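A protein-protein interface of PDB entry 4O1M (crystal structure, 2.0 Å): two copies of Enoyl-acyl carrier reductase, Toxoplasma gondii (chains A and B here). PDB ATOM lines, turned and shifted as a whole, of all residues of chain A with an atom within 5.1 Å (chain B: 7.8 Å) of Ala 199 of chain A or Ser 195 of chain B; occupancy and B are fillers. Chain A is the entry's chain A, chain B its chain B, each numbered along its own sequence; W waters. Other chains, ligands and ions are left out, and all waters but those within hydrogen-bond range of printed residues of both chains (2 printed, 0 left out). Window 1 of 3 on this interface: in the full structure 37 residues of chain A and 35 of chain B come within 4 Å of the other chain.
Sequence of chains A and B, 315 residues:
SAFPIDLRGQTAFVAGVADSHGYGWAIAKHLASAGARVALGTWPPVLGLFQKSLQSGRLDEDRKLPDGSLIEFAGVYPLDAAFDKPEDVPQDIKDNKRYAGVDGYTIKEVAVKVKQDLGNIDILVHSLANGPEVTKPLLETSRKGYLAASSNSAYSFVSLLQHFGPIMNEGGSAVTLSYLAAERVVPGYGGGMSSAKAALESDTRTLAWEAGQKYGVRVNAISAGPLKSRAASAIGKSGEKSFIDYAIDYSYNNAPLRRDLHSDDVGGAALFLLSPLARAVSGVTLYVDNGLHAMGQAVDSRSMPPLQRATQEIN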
ATOM      1  N   ALA A 154      26.214 -24.495 -36.599  1.00  0.00           N
ATOM      2  CA  ALA A 154      25.177 -24.305 -35.542  1.00  0.00           C
ATOM      3  C   ALA A 154      23.775 -24.436 -36.117  1.00  0.00           C
ATOM      4  O   ALA A 154      23.009 -25.299 -35.693  1.00  0.00           O
ATOM      5  CB  ALA A 154      25.351 -22.959 -34.805  1.00  0.00           C
ATOM      6  N   SER A 195      32.385 -19.009 -31.495  1.00  0.00           N
ATOM      7  CA  SER A 195      31.030 -18.400 -31.424  1.00  0.00           C
ATOM      8  C   SER A 195      29.957 -19.365 -31.907  1.00  0.00           C
ATOM      9  O   SER A 195      28.868 -19.434 -31.317  1.00  0.00           O
ATOM     10  CB  SER A 195      30.971 -17.128 -32.287  1.00  0.00           C
ATOM     11  OG  SER A 195      32.268 -16.576 -32.418  1.00  0.00           O
ATOM     12  N   ALA A 196      30.219 -20.044 -33.025  1.00  0.00           N
ATOM     13  CA  ALA A 196      29.279 -21.077 -33.497  1.00  0.00           C
ATOM     14  C   ALA A 196      29.073 -22.235 -32.494  1.00  0.00           C
ATOM     15  O   ALA A 196      27.958 -22.717 -32.350  1.00  0.00           O
ATOM     16  CB  ALA A 196      29.708 -21.625 -34.881  1.00  0.00           C
ATOM     17  N   LYS A 197      30.123 -22.678 -31.797  1.00  0.00           N
ATOM     18  CA  LYS A 197      29.951 -23.732 -30.809  1.00  0.00           C
ATOM     19  C   LYS A 197      29.177 -23.237 -29.589  1.00  0.00           C
ATOM     20  O   LYS A 197      28.395 -23.991 -29.012  1.00  0.00           O
ATOM     21  CB  LYS A 197      31.299 -24.331 -30.381  1.00  0.00           C
ATOM     22  CG  LYS A 197      32.035 -25.089 -31.509  1.00  0.00           C
ATOM     23  CD  LYS A 197      31.132 -26.173 -32.175  1.00  0.00           C
ATOM     24  CE  LYS A 197      31.987 -27.204 -32.972  1.00  0.00           C
ATOM     25  NZ  LYS A 197      31.219 -28.417 -33.467  1.00  0.00           N
ATOM     26  N   ALA A 198      29.380 -21.982 -29.191  1.00  0.00           N
ATOM     27  CA  ALA A 198      28.559 -21.392 -28.105  1.00  0.00           C
ATOM     28  C   ALA A 198      27.073 -21.348 -28.535  1.00  0.00           C
ATOM     29  O   ALA A 198      26.182 -21.671 -27.751  1.00  0.00           O
ATOM     30  CB  ALA A 198      29.062 -19.990 -27.764  1.00  0.00           C
ATOM     31  N   ALA A 199      26.820 -20.943 -29.786  1.00  0.00           N
ATOM     32  CA  ALA A 199      25.436 -20.929 -30.307  1.00  0.00           C
ATOM     33  C   ALA A 199      24.858 -22.351 -30.309  1.00  0.00           C
ATOM     34  O   ALA A 199      23.712 -22.548 -29.960  1.00  0.00           O
ATOM     35  CB  ALA A 199      25.382 -20.323 -31.738  1.00  0.00           C
ATOM     36  N   LEU A 200      25.678 -23.317 -30.737  1.00  0.00           N
ATOM     37  CA  LEU A 200      25.275 -24.720 -30.787  1.00  0.00           C
ATOM     38  C   LEU A 200      24.904 -25.286 -29.420  1.00  0.00           C
ATOM     39  O   LEU A 200      23.921 -26.014 -29.310  1.00  0.00           O
ATOM     40  CB  LEU A 200      26.404 -25.543 -31.402  1.00  0.00           C
ATOM     41  CG  LEU A 200      26.155 -27.051 -31.546  1.00  0.00           C
ATOM     42  CD1 LEU A 200      25.084 -27.372 -32.613  1.00  0.00           C
ATOM     43  CD2 LEU A 200      27.504 -27.692 -31.888  1.00  0.00           C
ATOM     44  N   GLU A 201      25.699 -24.984 -28.379  1.00  0.00           N
ATOM     45  CA  GLU A 201      25.387 -25.430 -27.009  1.00  0.00           C
ATOM     46  C   GLU A 201      24.141 -24.752 -26.491  1.00  0.00           C
ATOM     47  O   GLU A 201      23.359 -25.384 -25.789  1.00  0.00           O
ATOM     48  CB  GLU A 201      26.565 -25.203 -26.030  1.00  0.00           C
ATOM     49  CG  GLU A 201      27.801 -26.135 -26.360  1.00  0.00           C
ATOM     50  CD  GLU A 201      29.058 -25.897 -25.454  1.00  0.00           C
ATOM     51  OE1 GLU A 201      28.963 -25.128 -24.456  1.00  0.00           O
ATOM     52  OE2 GLU A 201      30.164 -26.447 -25.769  1.00  0.00           O
ATOM     53  N   SER A 202      23.964 -23.460 -26.808  1.00  0.00           N
ATOM     54  CA  SER A 202      22.718 -22.759 -26.408  1.00  0.00           C
ATOM     55  C   SER A 202      21.515 -23.399 -27.105  1.00  0.00           C
ATOM     56  O   SER A 202      20.501 -23.687 -26.454  1.00  0.00           O
ATOM     57  CB  SER A 202      22.779 -21.252 -26.736  1.00  0.00           C
ATOM     58  OG  SER A 202      21.512 -20.609 -26.490  1.00  0.00           O
ATOM     59  N   ASP A 203      21.613 -23.613 -28.422  1.00  0.00           N
ATOM     60  CA  ASP A 203      20.572 -24.348 -29.172  1.00  0.00           C
ATOM     61  C   ASP A 203      20.307 -25.770 -28.668  1.00  0.00           C
ATOM     62  O   ASP A 203      19.170 -26.246 -28.744  1.00  0.00           O
ATOM     63  CB  ASP A 203      20.844 -24.371 -30.678  1.00  0.00           C
ATOM     64  CG  ASP A 203      20.917 -22.962 -31.278  1.00  0.00           C
ATOM     65  OD1 ASP A 203      20.459 -21.991 -30.606  1.00  0.00           O
ATOM     66  OD2 ASP A 203      21.474 -22.815 -32.377  1.00  0.00           O
ATOM     67  N   THR A 204      21.325 -26.433 -28.121  1.00  0.00           N
ATOM     68  CA  THR A 204      21.113 -27.747 -27.510  1.00  0.00           C
ATOM     69  C   THR A 204      20.111 -27.643 -26.352  1.00  0.00           C
ATOM     70  O   THR A 204      19.166 -28.441 -26.245  1.00  0.00           O
ATOM     71  CB  THR A 204      22.450 -28.330 -27.030  1.00  0.00           C
ATOM     72  OG1 THR A 204      23.255 -28.624 -28.177  1.00  0.00           O
ATOM     73  CG2 THR A 204      22.224 -29.599 -26.220  1.00  0.00           C
ATOM     74  N   LEU B 138      12.575 -21.711 -32.086  1.00  0.00           N
ATOM     75  CA  LEU B 138      13.711 -22.209 -32.852  1.00  0.00           C
ATOM     76  C   LEU B 138      13.344 -23.333 -33.860  1.00  0.00           C
ATOM     77  O   LEU B 138      13.847 -23.333 -35.000  1.00  0.00           O
ATOM     78  CB  LEU B 138      14.837 -22.616 -31.878  1.00  0.00           C
ATOM     79  CG  LEU B 138      16.265 -22.659 -32.395  1.00  0.00           C
ATOM     80  CD1 LEU B 138      16.650 -21.332 -33.051  1.00  0.00           C
ATOM     81  CD2 LEU B 138      17.287 -23.012 -31.274  1.00  0.00           C
ATOM     82  N   THR B 141      12.257 -21.412 -36.975  1.00  0.00           N
ATOM     83  CA  THR B 141      13.109 -20.312 -37.428  1.00  0.00           C
ATOM     84  C   THR B 141      13.872 -20.740 -38.683  1.00  0.00           C
ATOM     85  O   THR B 141      14.462 -21.835 -38.733  1.00  0.00           O
ATOM     86  CB  THR B 141      14.080 -19.896 -36.276  1.00  0.00           C
ATOM     87  OG1 THR B 141      13.322 -19.407 -35.155  1.00  0.00           O
ATOM     88  CG2 THR B 141      15.076 -18.844 -36.719  1.00  0.00           C
ATOM     89  N   TYR B 146      17.736 -16.785 -38.721  1.00  0.00           N
ATOM     90  CA  TYR B 146      18.725 -17.128 -37.691  1.00  0.00           C
ATOM     91  C   TYR B 146      20.064 -16.411 -37.921  1.00  0.00           C
ATOM     92  O   TYR B 146      20.701 -15.862 -36.992  1.00  0.00           O
ATOM     93  CB  TYR B 146      18.967 -18.631 -37.773  1.00  0.00           C
ATOM     94  CG  TYR B 146      19.906 -19.217 -36.729  1.00  0.00           C
ATOM     95  CD1 TYR B 146      21.302 -19.307 -36.972  1.00  0.00           C
ATOM     96  CD2 TYR B 146      19.398 -19.761 -35.546  1.00  0.00           C
ATOM     97  CE1 TYR B 146      22.171 -19.892 -36.025  1.00  0.00           C
ATOM     98  CE2 TYR B 146      20.261 -20.362 -34.591  1.00  0.00           C
ATOM     99  CZ  TYR B 146      21.640 -20.428 -34.850  1.00  0.00           C
ATOM    100  OH  TYR B 146      22.464 -21.043 -33.923  1.00  0.00           O
ATOM    101  N   ALA B 149      19.806 -12.702 -37.205  1.00  0.00           N
ATOM    102  CA  ALA B 149      19.921 -12.409 -35.775  1.00  0.00           C
ATOM    103  C   ALA B 149      21.398 -12.371 -35.381  1.00  0.00           C
ATOM    104  O   ALA B 149      21.841 -11.476 -34.646  1.00  0.00           O
ATOM    105  CB  ALA B 149      19.187 -13.474 -34.928  1.00  0.00           C
ATOM    106  N   SER B 150      22.158 -13.354 -35.873  1.00  0.00           N
ATOM    107  CA  SER B 150      23.571 -13.442 -35.558  1.00  0.00           C
ATOM    108  C   SER B 150      24.354 -12.246 -36.166  1.00  0.00           C
ATOM    109  O   SER B 150      25.185 -11.661 -35.504  1.00  0.00           O
ATOM    110  CB  SER B 150      24.153 -14.748 -36.070  1.00  0.00           C
ATOM    111  OG  SER B 150      25.567 -14.706 -35.911  1.00  0.00           O
ATOM    112  N   ALA B 154      25.350 -10.306 -32.950  1.00  0.00           N
ATOM    113  CA  ALA B 154      26.624 -10.861 -32.435  1.00  0.00           C
ATOM    114  C   ALA B 154      27.812 -10.375 -33.256  1.00  0.00           C
ATOM    115  O   ALA B 154      28.713  -9.734 -32.739  1.00  0.00           O
ATOM    116  CB  ALA B 154      26.583 -12.433 -32.399  1.00  0.00           C
ATOM    117  N   ALA B 181      18.819 -15.747 -21.627  1.00  0.00           N
ATOM    118  CA  ALA B 181      18.447 -16.735 -22.661  1.00  0.00           C
ATOM    119  C   ALA B 181      19.685 -17.353 -23.360  1.00  0.00           C
ATOM    120  O   ALA B 181      19.578 -18.403 -23.950  1.00  0.00           O
ATOM    121  CB  ALA B 181      17.511 -16.072 -23.694  1.00  0.00           C
ATOM    122  N   ALA B 182      20.839 -16.671 -23.316  1.00  0.00           N
ATOM    123  CA  ALA B 182      22.096 -17.209 -23.837  1.00  0.00           C
ATOM    124  C   ALA B 182      22.555 -18.445 -23.090  1.00  0.00           C
ATOM    125  O   ALA B 182      23.216 -19.323 -23.683  1.00  0.00           O
ATOM    126  CB  ALA B 182      23.198 -16.161 -23.773  1.00  0.00           C
ATOM    127  N   TYR B 189      11.813 -16.014 -26.361  1.00  0.00           N
ATOM    128  CA  TYR B 189      12.966 -15.333 -26.946  1.00  0.00           C
ATOM    129  C   TYR B 189      13.515 -16.155 -28.111  1.00  0.00           C
ATOM    130  O   TYR B 189      14.552 -16.825 -27.990  1.00  0.00           O
ATOM    131  CB  TYR B 189      14.035 -15.081 -25.893  1.00  0.00           C
ATOM    132  CG  TYR B 189      15.058 -14.027 -26.275  1.00  0.00           C
ATOM    133  CD1 TYR B 189      14.663 -12.698 -26.547  1.00  0.00           C
ATOM    134  CD2 TYR B 189      16.424 -14.342 -26.339  1.00  0.00           C
ATOM    135  CE1 TYR B 189      15.604 -11.710 -26.854  1.00  0.00           C
ATOM    136  CE2 TYR B 189      17.390 -13.344 -26.633  1.00  0.00           C
ATOM    137  CZ  TYR B 189      16.974 -12.042 -26.891  1.00  0.00           C
ATOM    138  OH  TYR B 189      17.907 -11.077 -27.205  1.00  0.00           O
ATOM    139  N   GLY B 190      12.809 -16.099 -29.245  1.00  0.00           N
ATOM    140  CA  GLY B 190      13.070 -17.034 -30.353  1.00  0.00           C
ATOM    141  C   GLY B 190      13.903 -16.483 -31.491  1.00  0.00           C
ATOM    142  O   GLY B 190      14.720 -15.569 -31.291  1.00  0.00           O
ATOM    143  N   GLY B 191      13.707 -17.036 -32.686  1.00  0.00           N
ATOM    144  CA  GLY B 191      14.325 -16.479 -33.907  1.00  0.00           C
ATOM    145  C   GLY B 191      15.836 -16.623 -33.949  1.00  0.00           C
ATOM    146  O   GLY B 191      16.505 -15.994 -34.773  1.00  0.00           O
ATOM    147  N   GLY B 192      16.386 -17.482 -33.087  1.00  0.00           N
ATOM    148  CA  GLY B 192      17.841 -17.590 -32.990  1.00  0.00           C
ATOM    149  C   GLY B 192      18.501 -16.445 -32.219  1.00  0.00           C
ATOM    150  O   GLY B 192      19.749 -16.282 -32.272  1.00  0.00           O
ATOM    151  N   MET B 193      17.696 -15.600 -31.581  1.00  0.00           N
ATOM    152  CA  MET B 193      18.258 -14.540 -30.704  1.00  0.00           C
ATOM    153  C   MET B 193      18.928 -15.116 -29.458  1.00  0.00           C
ATOM    154  O   MET B 193      19.904 -14.541 -28.976  1.00  0.00           O
ATOM    155  CB  MET B 193      17.173 -13.545 -30.275  1.00  0.00           C
ATOM    156  CG  MET B 193      16.763 -12.560 -31.413  1.00  0.00           C
ATOM    157  SD  MET B 193      18.164 -11.555 -31.971  1.00  0.00           S
ATOM    158  CE  MET B 193      18.876 -10.895 -30.457  1.00  0.00           C
ATOM    159  N   SER B 194      18.428 -16.231 -28.919  1.00  0.00           N
ATOM    160  CA  SER B 194      19.155 -16.839 -27.766  1.00  0.00           C
ATOM    161  C   SER B 194      20.545 -17.298 -28.220  1.00  0.00           C
ATOM    162  O   SER B 194      21.559 -17.112 -27.512  1.00  0.00           O
ATOM    163  CB  SER B 194      18.354 -18.006 -27.157  1.00  0.00           C
ATOM    164  OG  SER B 194      18.077 -18.957 -28.165  1.00  0.00           O
ATOM    165  N   SER B 195      20.598 -17.859 -29.426  1.00  0.00           N
ATOM    166  CA  SER B 195      21.844 -18.396 -29.995  1.00  0.00           C
ATOM    167  C   SER B 195      22.804 -17.256 -30.270  1.00  0.00           C
ATOM    168  O   SER B 195      23.986 -17.357 -29.982  1.00  0.00           O
ATOM    169  CB  SER B 195      21.560 -19.172 -31.304  1.00  0.00           C
ATOM    170  OG  SER B 195      20.214 -19.642 -31.370  1.00  0.00           O
ATOM    171  N   ALA B 196      22.284 -16.141 -30.775  1.00  0.00           N
ATOM    172  CA  ALA B 196      23.118 -14.979 -31.029  1.00  0.00           C
ATOM    173  C   ALA B 196      23.657 -14.342 -29.753  1.00  0.00           C
ATOM    174  O   ALA B 196      24.840 -13.978 -29.719  1.00  0.00           O
ATOM    175  CB  ALA B 196      22.378 -13.921 -31.892  1.00  0.00           C
ATOM    176  N   LYS B 197      22.851 -14.262 -28.694  1.00  0.00           N
ATOM    177  CA  LYS B 197      23.373 -13.811 -27.412  1.00  0.00           C
ATOM    178  C   LYS B 197      24.444 -14.758 -26.818  1.00  0.00           C
ATOM    179  O   LYS B 197      25.423 -14.310 -26.202  1.00  0.00           O
ATOM    180  CB  LYS B 197      22.233 -13.584 -26.404  1.00  0.00           C
ATOM    181  CG  LYS B 197      21.293 -12.427 -26.805  1.00  0.00           C
ATOM    182  CD  LYS B 197      22.071 -11.105 -27.110  1.00  0.00           C
ATOM    183  CE  LYS B 197      21.051  -9.896 -27.045  1.00  0.00           C
ATOM    184  NZ  LYS B 197      21.741  -8.567 -27.106  1.00  0.00           N
ATOM    185  N   ALA B 198      24.279 -16.067 -26.975  1.00  0.00           N
ATOM    186  CA  ALA B 198      25.371 -16.983 -26.549  1.00  0.00           C
ATOM    187  C   ALA B 198      26.701 -16.731 -27.317  1.00  0.00           C
ATOM    188  O   ALA B 198      27.792 -16.755 -26.745  1.00  0.00           O
ATOM    189  CB  ALA B 198      24.931 -18.421 -26.737  1.00  0.00           C
ATOM    190  N   ALA B 199      26.591 -16.517 -28.622  1.00  0.00           N
ATOM    191  CA  ALA B 199      27.762 -16.253 -29.469  1.00  0.00           C
ATOM    192  C   ALA B 199      28.353 -14.922 -29.036  1.00  0.00           C
ATOM    193  O   ALA B 199      29.579 -14.766 -28.978  1.00  0.00           O
ATOM    194  CB  ALA B 199      27.327 -16.174 -30.961  1.00  0.00           C
ATOM    195  N   LEU B 200      27.488 -13.948 -28.738  1.00  0.00           N
ATOM    196  CA  LEU B 200      27.950 -12.639 -28.234  1.00  0.00           C
ATOM    197  C   LEU B 200      28.734 -12.728 -26.908  1.00  0.00           C
ATOM    198  O   LEU B 200      29.764 -12.032 -26.759  1.00  0.00           O
ATOM    199  CB  LEU B 200      26.781 -11.681 -28.080  1.00  0.00           C
ATOM    200  CG  LEU B 200      27.068 -10.248 -27.647  1.00  0.00           C
ATOM    201  CD1 LEU B 200      27.813  -9.460 -28.758  1.00  0.00           C
ATOM    202  CD2 LEU B 200      25.744  -9.581 -27.316  1.00  0.00           C
ATOM    203  N   GLU B 201      28.243 -13.514 -25.947  1.00  0.00           N
ATOM    204  CA  GLU B 201      28.999 -13.717 -24.683  1.00  0.00           C
ATOM    205  C   GLU B 201      30.329 -14.453 -24.923  1.00  0.00           C
ATOM    206  O   GLU B 201      31.349 -14.136 -24.336  1.00  0.00           O
ATOM    207  CB  GLU B 201      28.136 -14.460 -23.624  1.00  0.00           C
ATOM    208  CG  GLU B 201      26.932 -13.543 -23.177  1.00  0.00           C
ATOM    209  CD  GLU B 201      25.967 -14.218 -22.146  1.00  0.00           C
ATOM    210  OE1 GLU B 201      26.314 -15.291 -21.590  1.00  0.00           O
ATOM    211  OE2 GLU B 201      24.855 -13.684 -21.877  1.00  0.00           O
ATOM    212  N   SER B 202      30.316 -15.436 -25.811  1.00  0.00           N
ATOM    213  CA  SER B 202      31.552 -16.166 -26.126  1.00  0.00           C
ATOM    214  C   SER B 202      32.563 -15.188 -26.776  1.00  0.00           C
ATOM    215  O   SER B 202      33.770 -15.190 -26.456  1.00  0.00           O
ATOM    216  CB  SER B 202      31.219 -17.332 -27.066  1.00  0.00           C
ATOM    217  OG  SER B 202      32.432 -17.929 -27.536  1.00  0.00           O
HETATM  218  O   HOH W   1      19.539 -21.125 -28.103  1.00  0.00           O
HETATM  219  O   HOH W   2      20.590 -21.294 -23.717  1.00  0.00           O
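The side-chain hydroxyl of Tyr 146 of chain B sits at hydrogen-bond distance from the side-chain carboxylate of Asp 203 of chain A (2.6 Å). The side-chain carboxylate of Asp 203 of chain A sits at hydrogen-bond distance from the side-chain hydroxyl of Ser 195 of chain B, 2.5 Å away.
Among the printed residues, merely in contact across the chains: Ala 154 of chain A with Tyr 146 of chain B (3.6 Å), Ser 195 of chain A with Ala 199 of chain B (3.6 Å), Ala 198 of chain A with Ala 198 of chain B (3.6 Å), Ala 198 of chain A with Ser 202 of chain B (3.5 Å), Ala 199 of chain A with Tyr 146 of chain B (3.7 Å), Ala 199 of chain A with Ser 195 of chain B (3.7 Å), Ser 202 of chain A with Ala 181 of chain B (3.9 Å), Ser 202 of chain A with Ala 182 of chain B (3.5 Å), Ser 202 of chain A with Ser 194 of chain B (3.6 Å), Ser 202 of chain A with Ala 198 of chain B (3.6 Å) and Asp 203 of chain A with Leu 138 of chain B (3.4 Å).
Of the printed residues of chain B, Ala 154 of chain A touches Tyr 146 (3.6 Å). Of the printed residues of chain B, Ser 195 of chain A touches Ala 199. Ala 196 of chain A touches none of the printed residues of chain B. Ala 199 of chain A touches just these residues of chain B: Tyr 146 and Ser 195. Glu 201 of chain A touches none of the printed residues of chain B. Of the printed residues of chain B, Ser 202 of chain A touches Ala 181, Ala 182, Ser 194 and Ala 198. Printed residues of chain A within 4 Å of Ser 194 of chain B: Ser 202. Printed residues of chain A within 4 Å of Ala 198 of chain B: Ala 198 (3.6 Å) and Ser 202 (3.6 Å). The nearest printed residue of chain A that does not touch Tyr 146 of chain B is Leu 200 of chain A (5.1 Å).
Printed residues of chain A that touch a printed residue of chain B: Ala 154, Ser 195, Ala 198, Ala 199, Ser 202 and Asp 203. Hydrophobic or aromatic side chains of chain A that line the printed part of chain B: Ala 154, Ala 198 and Ala 199. Along chain A the printed residues that touch a printed residue of chain B span positions 154 to 203. Among the printed residues, no Asp or Glu carboxylate lies within 4 Å of a Lys or Arg side-chain nitrogen of the other chain.
Ser 195 of chain A touches Ala 199 of chain B, and with the chains exchanged Ala 199 of chain A touches Ser 195 of chain B. Ala 198 of chain B touches its own counterpart, Ala 198 of chain A. Ala 198 of chain A touches Ser 202 of chain B, and with the chains exchanged Ser 202 of chain A touches Ala 198 of chain B. Of the 13 pairs that touch across the chains among the printed residues, 5 have their exchanged pair printed and touching as well.
Water W1 lies within hydrogen-bond range of the side-chain hydroxyl (OG) of Ser 202 of chain A (2.6 Å), the side-chain hydroxyl (OG) of Ser 194 of chain B (2.6 Å) and the side-chain carboxylate (OD1) of Asp 203 of chain A (2.8 Å). Water W2 lies within hydrogen-bond range of OG of Ser 202 of chain A (3.0 Å), O of Ala 181 of chain B (3.1 Å) and O of Ala 182 of chain B (3.3 Å).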
